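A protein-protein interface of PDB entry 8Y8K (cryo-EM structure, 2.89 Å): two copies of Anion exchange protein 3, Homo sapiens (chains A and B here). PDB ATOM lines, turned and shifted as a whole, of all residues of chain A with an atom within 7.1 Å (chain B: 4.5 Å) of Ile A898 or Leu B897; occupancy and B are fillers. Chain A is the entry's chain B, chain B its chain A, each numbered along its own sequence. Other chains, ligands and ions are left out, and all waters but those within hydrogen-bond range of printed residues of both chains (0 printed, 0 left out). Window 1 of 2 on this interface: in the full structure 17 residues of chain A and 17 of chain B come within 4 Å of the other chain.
Of the printed residues of chain B, Ile A898 touches Leu B894 and Leu B897. Leu B897 touches one residue of chain A. Printed residues of chain A within 4 Å of Leu B894: Ile A898 (3.7 Å). Of the printed residues of chain B, Leu A897 touches Ile B898. Printed residues of chain B within 4 Å of Leu A894: Ile B898. Printed residues of chain A within 4 Å of Ile B898: Leu A894 and Leu A897. Ala B893 touches none of the printed residues of chain A. Leu B895 touches none of the printed residues of chain A. The nearest printed residue of chain A that does not touch Leu B897 is Leu A895 (7.5 Å). The nearest printed residue of chain A that does not touch Ile B898 is Ile A898 (4.04 Å).
Ile B898 touches Leu A894. CD1 of Ile B898 touches CD2 of Leu A897 (3.9 Å). Ile A898 touches Leu B894 (CD1 to CD2, 3.7 Å). Leu B897 touches Ile A898 (CD2 to CD1, 3.9 Å).
Leu A894 touches Ile B898, and with the chains exchanged Ile A898 touches Leu B894. Leu A897 touches Ile B898, and with the chains exchanged Ile A898 touches Leu B897. 10 positions are printed for both chains. Of the 4 pairs that touch across the chains among the printed residues, 4 have their exchanged pair printed and touching as well.
Of the 10 printed residues of chain B, 3 touch a printed residue of chain A. Hydrophobic or aromatic side chains of chain B that line the printed part of chain A: Leu B894, Leu B897 and Ile B898. Printed residues of chain A that touch a printed residue of chain B: Leu A894, Leu A897 and Ile A898. Hydrophobic or aromatic side chains of chain A that line the printed part of chain B: Leu A894, Leu A897 and Ile A898. Among the printed residues, 4 pairs touch across the chains.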
ATOM      1  N   LEU A 843     -17.504  28.290 -14.304  1.00  0.00           N
ATOM      2  CA  LEU A 843     -18.183  27.517 -13.261  1.00  0.00           C
ATOM      3  C   LEU A 843     -17.932  26.016 -13.420  1.00  0.00           C
ATOM      4  O   LEU A 843     -17.685  25.302 -12.433  1.00  0.00           O
ATOM      5  CB  LEU A 843     -19.682  27.811 -13.271  1.00  0.00           C
ATOM      6  CG  LEU A 843     -20.522  27.077 -12.221  1.00  0.00           C
ATOM      7  CD1 LEU A 843     -20.258  27.621 -10.828  1.00  0.00           C
ATOM      8  CD2 LEU A 843     -21.997  27.152 -12.557  1.00  0.00           C
ATOM      9  N   PHE A 847     -16.181  23.162 -10.882  1.00  0.00           N
ATOM     10  CA  PHE A 847     -16.696  21.851 -10.487  1.00  0.00           C
ATOM     11  C   PHE A 847     -15.683  20.740 -10.749  1.00  0.00           C
ATOM     12  O   PHE A 847     -15.549  19.817  -9.941  1.00  0.00           O
ATOM     13  CB  PHE A 847     -18.014  21.528 -11.193  1.00  0.00           C
ATOM     14  CG  PHE A 847     -19.225  22.092 -10.508  1.00  0.00           C
ATOM     15  CD1 PHE A 847     -19.182  23.324  -9.888  1.00  0.00           C
ATOM     16  CD2 PHE A 847     -20.382  21.345 -10.409  1.00  0.00           C
ATOM     17  CE1 PHE A 847     -20.292  23.828  -9.247  1.00  0.00           C
ATOM     18  CE2 PHE A 847     -21.490  21.842  -9.757  1.00  0.00           C
ATOM     19  CZ  PHE A 847     -21.443  23.083  -9.175  1.00  0.00           C
ATOM     20  N   ALA A 893     -17.852  23.042  -4.635  1.00  0.00           N
ATOM     21  CA  ALA A 893     -18.516  23.285  -5.911  1.00  0.00           C
ATOM     22  C   ALA A 893     -19.956  23.748  -5.713  1.00  0.00           C
ATOM     23  O   ALA A 893     -20.396  24.737  -6.319  1.00  0.00           O
ATOM     24  CB  ALA A 893     -18.466  22.021  -6.762  1.00  0.00           C
ATOM     25  N   LEU A 894     -20.711  23.041  -4.868  1.00  0.00           N
ATOM     26  CA  LEU A 894     -22.124  23.358  -4.681  1.00  0.00           C
ATOM     27  C   LEU A 894     -22.312  24.734  -4.057  1.00  0.00           C
ATOM     28  O   LEU A 894     -23.235  25.470  -4.425  1.00  0.00           O
ATOM     29  CB  LEU A 894     -22.792  22.282  -3.827  1.00  0.00           C
ATOM     30  CG  LEU A 894     -22.828  20.869  -4.411  1.00  0.00           C
ATOM     31  CD1 LEU A 894     -23.293  19.889  -3.366  1.00  0.00           C
ATOM     32  CD2 LEU A 894     -23.725  20.804  -5.631  1.00  0.00           C
ATOM     33  N   LEU A 895     -21.451  25.099  -3.109  1.00  0.00           N
ATOM     34  CA  LEU A 895     -21.518  26.434  -2.531  1.00  0.00           C
ATOM     35  C   LEU A 895     -21.238  27.504  -3.578  1.00  0.00           C
ATOM     36  O   LEU A 895     -21.855  28.574  -3.559  1.00  0.00           O
ATOM     37  CB  LEU A 895     -20.539  26.550  -1.367  1.00  0.00           C
ATOM     38  CG  LEU A 895     -20.650  27.836  -0.552  1.00  0.00           C
ATOM     39  CD1 LEU A 895     -22.017  27.939   0.095  1.00  0.00           C
ATOM     40  CD2 LEU A 895     -19.553  27.903   0.488  1.00  0.00           C
ATOM     41  N   SER A 896     -20.304  27.239  -4.494  1.00  0.00           N
ATOM     42  CA  SER A 896     -20.026  28.187  -5.567  1.00  0.00           C
ATOM     43  C   SER A 896     -21.241  28.377  -6.464  1.00  0.00           C
ATOM     44  O   SER A 896     -21.589  29.512  -6.824  1.00  0.00           O
ATOM     45  CB  SER A 896     -18.829  27.709  -6.386  1.00  0.00           C
ATOM     46  OG  SER A 896     -17.687  27.549  -5.569  1.00  0.00           O
ATOM     47  N   LEU A 897     -21.899  27.277  -6.833  1.00  0.00           N
ATOM     48  CA  LEU A 897     -23.113  27.375  -7.637  1.00  0.00           C
ATOM     49  C   LEU A 897     -24.188  28.178  -6.912  1.00  0.00           C
ATOM     50  O   LEU A 897     -24.856  29.032  -7.514  1.00  0.00           O
ATOM     51  CB  LEU A 897     -23.615  25.973  -7.975  1.00  0.00           C
ATOM     52  CG  LEU A 897     -24.934  25.812  -8.724  1.00  0.00           C
ATOM     53  CD1 LEU A 897     -24.806  26.335 -10.142  1.00  0.00           C
ATOM     54  CD2 LEU A 897     -25.360  24.357  -8.728  1.00  0.00           C
ATOM     55  N   ILE A 898     -24.355  27.928  -5.613  1.00  0.00           N
ATOM     56  CA  ILE A 898     -25.363  28.641  -4.836  1.00  0.00           C
ATOM     57  C   ILE A 898     -25.063  30.134  -4.800  1.00  0.00           C
ATOM     58  O   ILE A 898     -25.960  30.963  -4.987  1.00  0.00           O
ATOM     59  CB  ILE A 898     -25.462  28.045  -3.419  1.00  0.00           C
ATOM     60  CG1 ILE A 898     -26.202  26.708  -3.459  1.00  0.00           C
ATOM     61  CG2 ILE A 898     -26.161  29.003  -2.477  1.00  0.00           C
ATOM     62  CD1 ILE A 898     -26.151  25.948  -2.168  1.00  0.00           C
ATOM     63  N   LEU A 899     -23.801  30.503  -4.562  1.00  0.00           N
ATOM     64  CA  LEU A 899     -23.441  31.919  -4.497  1.00  0.00           C
ATOM     65  C   LEU A 899     -23.679  32.617  -5.830  1.00  0.00           C
ATOM     66  O   LEU A 899     -24.234  33.725  -5.874  1.00  0.00           O
ATOM     67  CB  LEU A 899     -21.981  32.074  -4.072  1.00  0.00           C
ATOM     68  CG  LEU A 899     -21.600  31.740  -2.631  1.00  0.00           C
ATOM     69  CD1 LEU A 899     -20.109  31.925  -2.428  1.00  0.00           C
ATOM     70  CD2 LEU A 899     -22.381  32.584  -1.647  1.00  0.00           C
ATOM     71  N   MET A 900     -23.273  31.980  -6.929  1.00  0.00           N
ATOM     72  CA  MET A 900     -23.463  32.577  -8.247  1.00  0.00           C
ATOM     73  C   MET A 900     -24.942  32.809  -8.545  1.00  0.00           C
ATOM     74  O   MET A 900     -25.351  33.918  -8.930  1.00  0.00           O
ATOM     75  CB  MET A 900     -22.817  31.679  -9.303  1.00  0.00           C
ATOM     76  CG  MET A 900     -23.479  31.686 -10.659  1.00  0.00           C
ATOM     77  SD  MET A 900     -22.461  30.830 -11.871  1.00  0.00           S
ATOM     78  CE  MET A 900     -23.083  31.523 -13.395  1.00  0.00           C
ATOM     79  N   LEU A 901     -25.770  31.779  -8.340  1.00  0.00           N
ATOM     80  CA  LEU A 901     -27.188  31.909  -8.661  1.00  0.00           C
ATOM     81  C   LEU A 901     -27.882  32.901  -7.734  1.00  0.00           C
ATOM     82  O   LEU A 901     -28.761  33.655  -8.170  1.00  0.00           O
ATOM     83  CB  LEU A 901     -27.869  30.545  -8.603  1.00  0.00           C
ATOM     84  CG  LEU A 901     -27.554  29.627  -9.786  1.00  0.00           C
ATOM     85  CD1 LEU A 901     -28.454  28.409  -9.775  1.00  0.00           C
ATOM     86  CD2 LEU A 901     -27.682  30.383 -11.099  1.00  0.00           C
ATOM     87  N   GLY A 902     -27.502  32.922  -6.456  1.00  0.00           N
ATOM     88  CA  GLY A 902     -28.090  33.881  -5.541  1.00  0.00           C
ATOM     89  C   GLY A 902     -27.799  35.314  -5.930  1.00  0.00           C
ATOM     90  O   GLY A 902     -28.695  36.162  -5.917  1.00  0.00           O
ATOM     91  N   THR A 903     -26.545  35.608  -6.289  1.00  0.00           N
ATOM     92  CA  THR A 903     -26.209  36.966  -6.712  1.00  0.00           C
ATOM     93  C   THR A 903     -27.001  37.363  -7.952  1.00  0.00           C
ATOM     94  O   THR A 903     -27.592  38.454  -8.006  1.00  0.00           O
ATOM     95  CB  THR A 903     -24.710  37.083  -6.978  1.00  0.00           C
ATOM     96  OG1 THR A 903     -23.986  36.509  -5.887  1.00  0.00           O
ATOM     97  CG2 THR A 903     -24.310  38.533  -7.114  1.00  0.00           C
ATOM     98  N   PHE A 904     -27.044  36.475  -8.953  1.00  0.00           N
ATOM     99  CA  PHE A 904     -27.776  36.792 -10.176  1.00  0.00           C
ATOM    100  C   PHE A 904     -29.247  37.073  -9.892  1.00  0.00           C
ATOM    101  O   PHE A 904     -29.803  38.070 -10.374  1.00  0.00           O
ATOM    102  CB  PHE A 904     -27.638  35.650 -11.179  1.00  0.00           C
ATOM    103  CG  PHE A 904     -28.473  35.822 -12.413  1.00  0.00           C
ATOM    104  CD1 PHE A 904     -28.132  36.754 -13.373  1.00  0.00           C
ATOM    105  CD2 PHE A 904     -29.594  35.041 -12.619  1.00  0.00           C
ATOM    106  CE1 PHE A 904     -28.896  36.908 -14.513  1.00  0.00           C
ATOM    107  CE2 PHE A 904     -30.360  35.191 -13.758  1.00  0.00           C
ATOM    108  CZ  PHE A 904     -30.010  36.126 -14.705  1.00  0.00           C
ATOM    109  N   MET A 939     -24.222  38.743  -0.829  1.00  0.00           N
ATOM    110  CA  MET A 939     -23.636  37.426  -1.053  1.00  0.00           C
ATOM    111  C   MET A 939     -22.243  37.311  -0.444  1.00  0.00           C
ATOM    112  O   MET A 939     -21.861  36.230   0.016  1.00  0.00           O
ATOM    113  CB  MET A 939     -23.612  37.109  -2.545  1.00  0.00           C
ATOM    114  CG  MET A 939     -24.206  35.754  -2.864  1.00  0.00           C
ATOM    115  SD  MET A 939     -25.931  35.639  -2.353  1.00  0.00           S
ATOM    116  CE  MET A 939     -26.070  33.891  -1.996  1.00  0.00           C
ATOM    117  N   VAL A 942     -22.913  36.602   3.186  1.00  0.00           N
ATOM    118  CA  VAL A 942     -23.355  35.219   3.345  1.00  0.00           C
ATOM    119  C   VAL A 942     -22.168  34.268   3.268  1.00  0.00           C
ATOM    120  O   VAL A 942     -22.039  33.346   4.081  1.00  0.00           O
ATOM    121  CB  VAL A 942     -24.427  34.875   2.294  1.00  0.00           C
ATOM    122  CG1 VAL A 942     -24.530  33.375   2.106  1.00  0.00           C
ATOM    123  CG2 VAL A 942     -25.767  35.456   2.703  1.00  0.00           C
ATOM    124  N   ALA A1108     -17.487  33.471  -7.194  1.00  0.00           N
ATOM    125  CA  ALA A1108     -18.821  33.091  -7.646  1.00  0.00           C
ATOM    126  C   ALA A1108     -19.761  34.289  -7.691  1.00  0.00           C
ATOM    127  O   ALA A1108     -20.634  34.365  -8.568  1.00  0.00           O
ATOM    128  CB  ALA A1108     -19.382  31.998  -6.743  1.00  0.00           C
ATOM    129  N   LEU B 843     -36.653  21.441   6.032  1.00  0.00           N
ATOM    130  CA  LEU B 843     -35.407  21.678   5.301  1.00  0.00           C
ATOM    131  C   LEU B 843     -34.247  21.949   6.254  1.00  0.00           C
ATOM    132  O   LEU B 843     -33.139  21.441   6.054  1.00  0.00           O
ATOM    133  CB  LEU B 843     -35.564  22.844   4.328  1.00  0.00           C
ATOM    134  CG  LEU B 843     -34.242  23.330   3.719  1.00  0.00           C
ATOM    135  CD1 LEU B 843     -33.685  22.323   2.726  1.00  0.00           C
ATOM    136  CD2 LEU B 843     -34.391  24.699   3.081  1.00  0.00           C
ATOM    137  N   ALA B 893     -26.499  18.369   2.520  1.00  0.00           N
ATOM    138  CA  ALA B 893     -27.416  19.465   2.815  1.00  0.00           C
ATOM    139  C   ALA B 893     -27.536  20.431   1.641  1.00  0.00           C
ATOM    140  O   ALA B 893     -28.645  20.856   1.284  1.00  0.00           O
ATOM    141  CB  ALA B 893     -26.954  20.197   4.069  1.00  0.00           C
ATOM    142  N   LEU B 894     -26.406  20.798   1.031  1.00  0.00           N
ATOM    143  CA  LEU B 894     -26.428  21.758  -0.070  1.00  0.00           C
ATOM    144  C   LEU B 894     -27.165  21.201  -1.281  1.00  0.00           C
ATOM    145  O   LEU B 894     -27.902  21.928  -1.958  1.00  0.00           O
ATOM    146  CB  LEU B 894     -25.004  22.162  -0.442  1.00  0.00           C
ATOM    147  CG  LEU B 894     -24.199  22.912   0.620  1.00  0.00           C
ATOM    148  CD1 LEU B 894     -22.764  23.044   0.185  1.00  0.00           C
ATOM    149  CD2 LEU B 894     -24.795  24.275   0.897  1.00  0.00           C
ATOM    150  N   LEU B 895     -26.977  19.916  -1.573  1.00  0.00           N
ATOM    151  CA  LEU B 895     -27.716  19.293  -2.663  1.00  0.00           C
ATOM    152  C   LEU B 895     -29.213  19.287  -2.381  1.00  0.00           C
ATOM    153  O   LEU B 895     -30.022  19.465  -3.298  1.00  0.00           O
ATOM    154  CB  LEU B 895     -27.207  17.874  -2.898  1.00  0.00           C
ATOM    155  CG  LEU B 895     -27.765  17.179  -4.136  1.00  0.00           C
ATOM    156  CD1 LEU B 895     -27.361  17.927  -5.393  1.00  0.00           C
ATOM    157  CD2 LEU B 895     -27.302  15.740  -4.190  1.00  0.00           C
ATOM    158  N   SER B 896     -29.601  19.074  -1.122  1.00  0.00           N
ATOM    159  CA  SER B 896     -31.014  19.121  -0.763  1.00  0.00           C
ATOM    160  C   SER B 896     -31.597  20.507  -0.999  1.00  0.00           C
ATOM    161  O   SER B 896     -32.699  20.643  -1.552  1.00  0.00           O
ATOM    162  CB  SER B 896     -31.194  18.709   0.697  1.00  0.00           C
ATOM    163  OG  SER B 896     -30.656  17.421   0.929  1.00  0.00           O
ATOM    164  N   LEU B 897     -30.873  21.547  -0.585  1.00  0.00           N
ATOM    165  CA  LEU B 897     -31.327  22.912  -0.833  1.00  0.00           C
ATOM    166  C   LEU B 897     -31.471  23.180  -2.327  1.00  0.00           C
ATOM    167  O   LEU B 897     -32.460  23.780  -2.773  1.00  0.00           O
ATOM    168  CB  LEU B 897     -30.350  23.896  -0.194  1.00  0.00           C
ATOM    169  CG  LEU B 897     -30.551  25.394  -0.406  1.00  0.00           C
ATOM    170  CD1 LEU B 897     -31.809  25.864   0.301  1.00  0.00           C
ATOM    171  CD2 LEU B 897     -29.342  26.160   0.093  1.00  0.00           C
ATOM    172  N   ILE B 898     -30.498  22.723  -3.119  1.00  0.00           N
ATOM    173  CA  ILE B 898     -30.545  22.937  -4.562  1.00  0.00           C
ATOM    174  C   ILE B 898     -31.758  22.245  -5.172  1.00  0.00           C
ATOM    175  O   ILE B 898     -32.469  22.827  -5.998  1.00  0.00           O
ATOM    176  CB  ILE B 898     -29.231  22.464  -5.212  1.00  0.00           C
ATOM    177  CG1 ILE B 898     -28.113  23.466  -4.930  1.00  0.00           C
ATOM    178  CG2 ILE B 898     -29.404  22.278  -6.705  1.00  0.00           C
ATOM    179  CD1 ILE B 898     -26.753  22.984  -5.334  1.00  0.00           C
ATOM    180  N   LEU B 899     -32.018  20.994  -4.777  1.00  0.00           N
ATOM    181  CA  LEU B 899     -33.154  20.261  -5.333  1.00  0.00           C
ATOM    182  C   LEU B 899     -34.477  20.931  -4.979  1.00  0.00           C
ATOM    183  O   LEU B 899     -35.359  21.080  -5.839  1.00  0.00           O
ATOM    184  CB  LEU B 899     -33.147  18.815  -4.840  1.00  0.00           C
ATOM    185  CG  LEU B 899     -32.059  17.876  -5.357  1.00  0.00           C
ATOM    186  CD1 LEU B 899     -32.196  16.511  -4.709  1.00  0.00           C
ATOM    187  CD2 LEU B 899     -32.109  17.760  -6.862  1.00  0.00           C
ATOM    188  N   MET B 900     -34.630  21.347  -3.721  1.00  0.00           N
ATOM    189  CA  MET B 900     -35.866  21.998  -3.301  1.00  0.00           C
ATOM    190  C   MET B 900     -36.112  23.283  -4.089  1.00  0.00           C
ATOM    191  O   MET B 900     -37.206  23.492  -4.644  1.00  0.00           O
ATOM    192  CB  MET B 900     -35.804  22.270  -1.798  1.00  0.00           C
ATOM    193  CG  MET B 900     -36.539  23.503  -1.328  1.00  0.00           C
ATOM    194  SD  MET B 900     -36.632  23.547   0.468  1.00  0.00           S
ATOM    195  CE  MET B 900     -38.032  24.628   0.715  1.00  0.00           C
ATOM    196  N   LEU B 901     -35.095  24.145  -4.177  1.00  0.00           N
ATOM    197  CA  LEU B 901     -35.276  25.419  -4.868  1.00  0.00           C
ATOM    198  C   LEU B 901     -35.491  25.218  -6.364  1.00  0.00           C
ATOM    199  O   LEU B 901     -36.288  25.933  -6.983  1.00  0.00           O
ATOM    200  CB  LEU B 901     -34.083  26.334  -4.608  1.00  0.00           C
ATOM    201  CG  LEU B 901     -34.035  26.930  -3.201  1.00  0.00           C
ATOM    202  CD1 LEU B 901     -32.961  27.995  -3.106  1.00  0.00           C
ATOM    203  CD2 LEU B 901     -35.390  27.493  -2.812  1.00  0.00           C
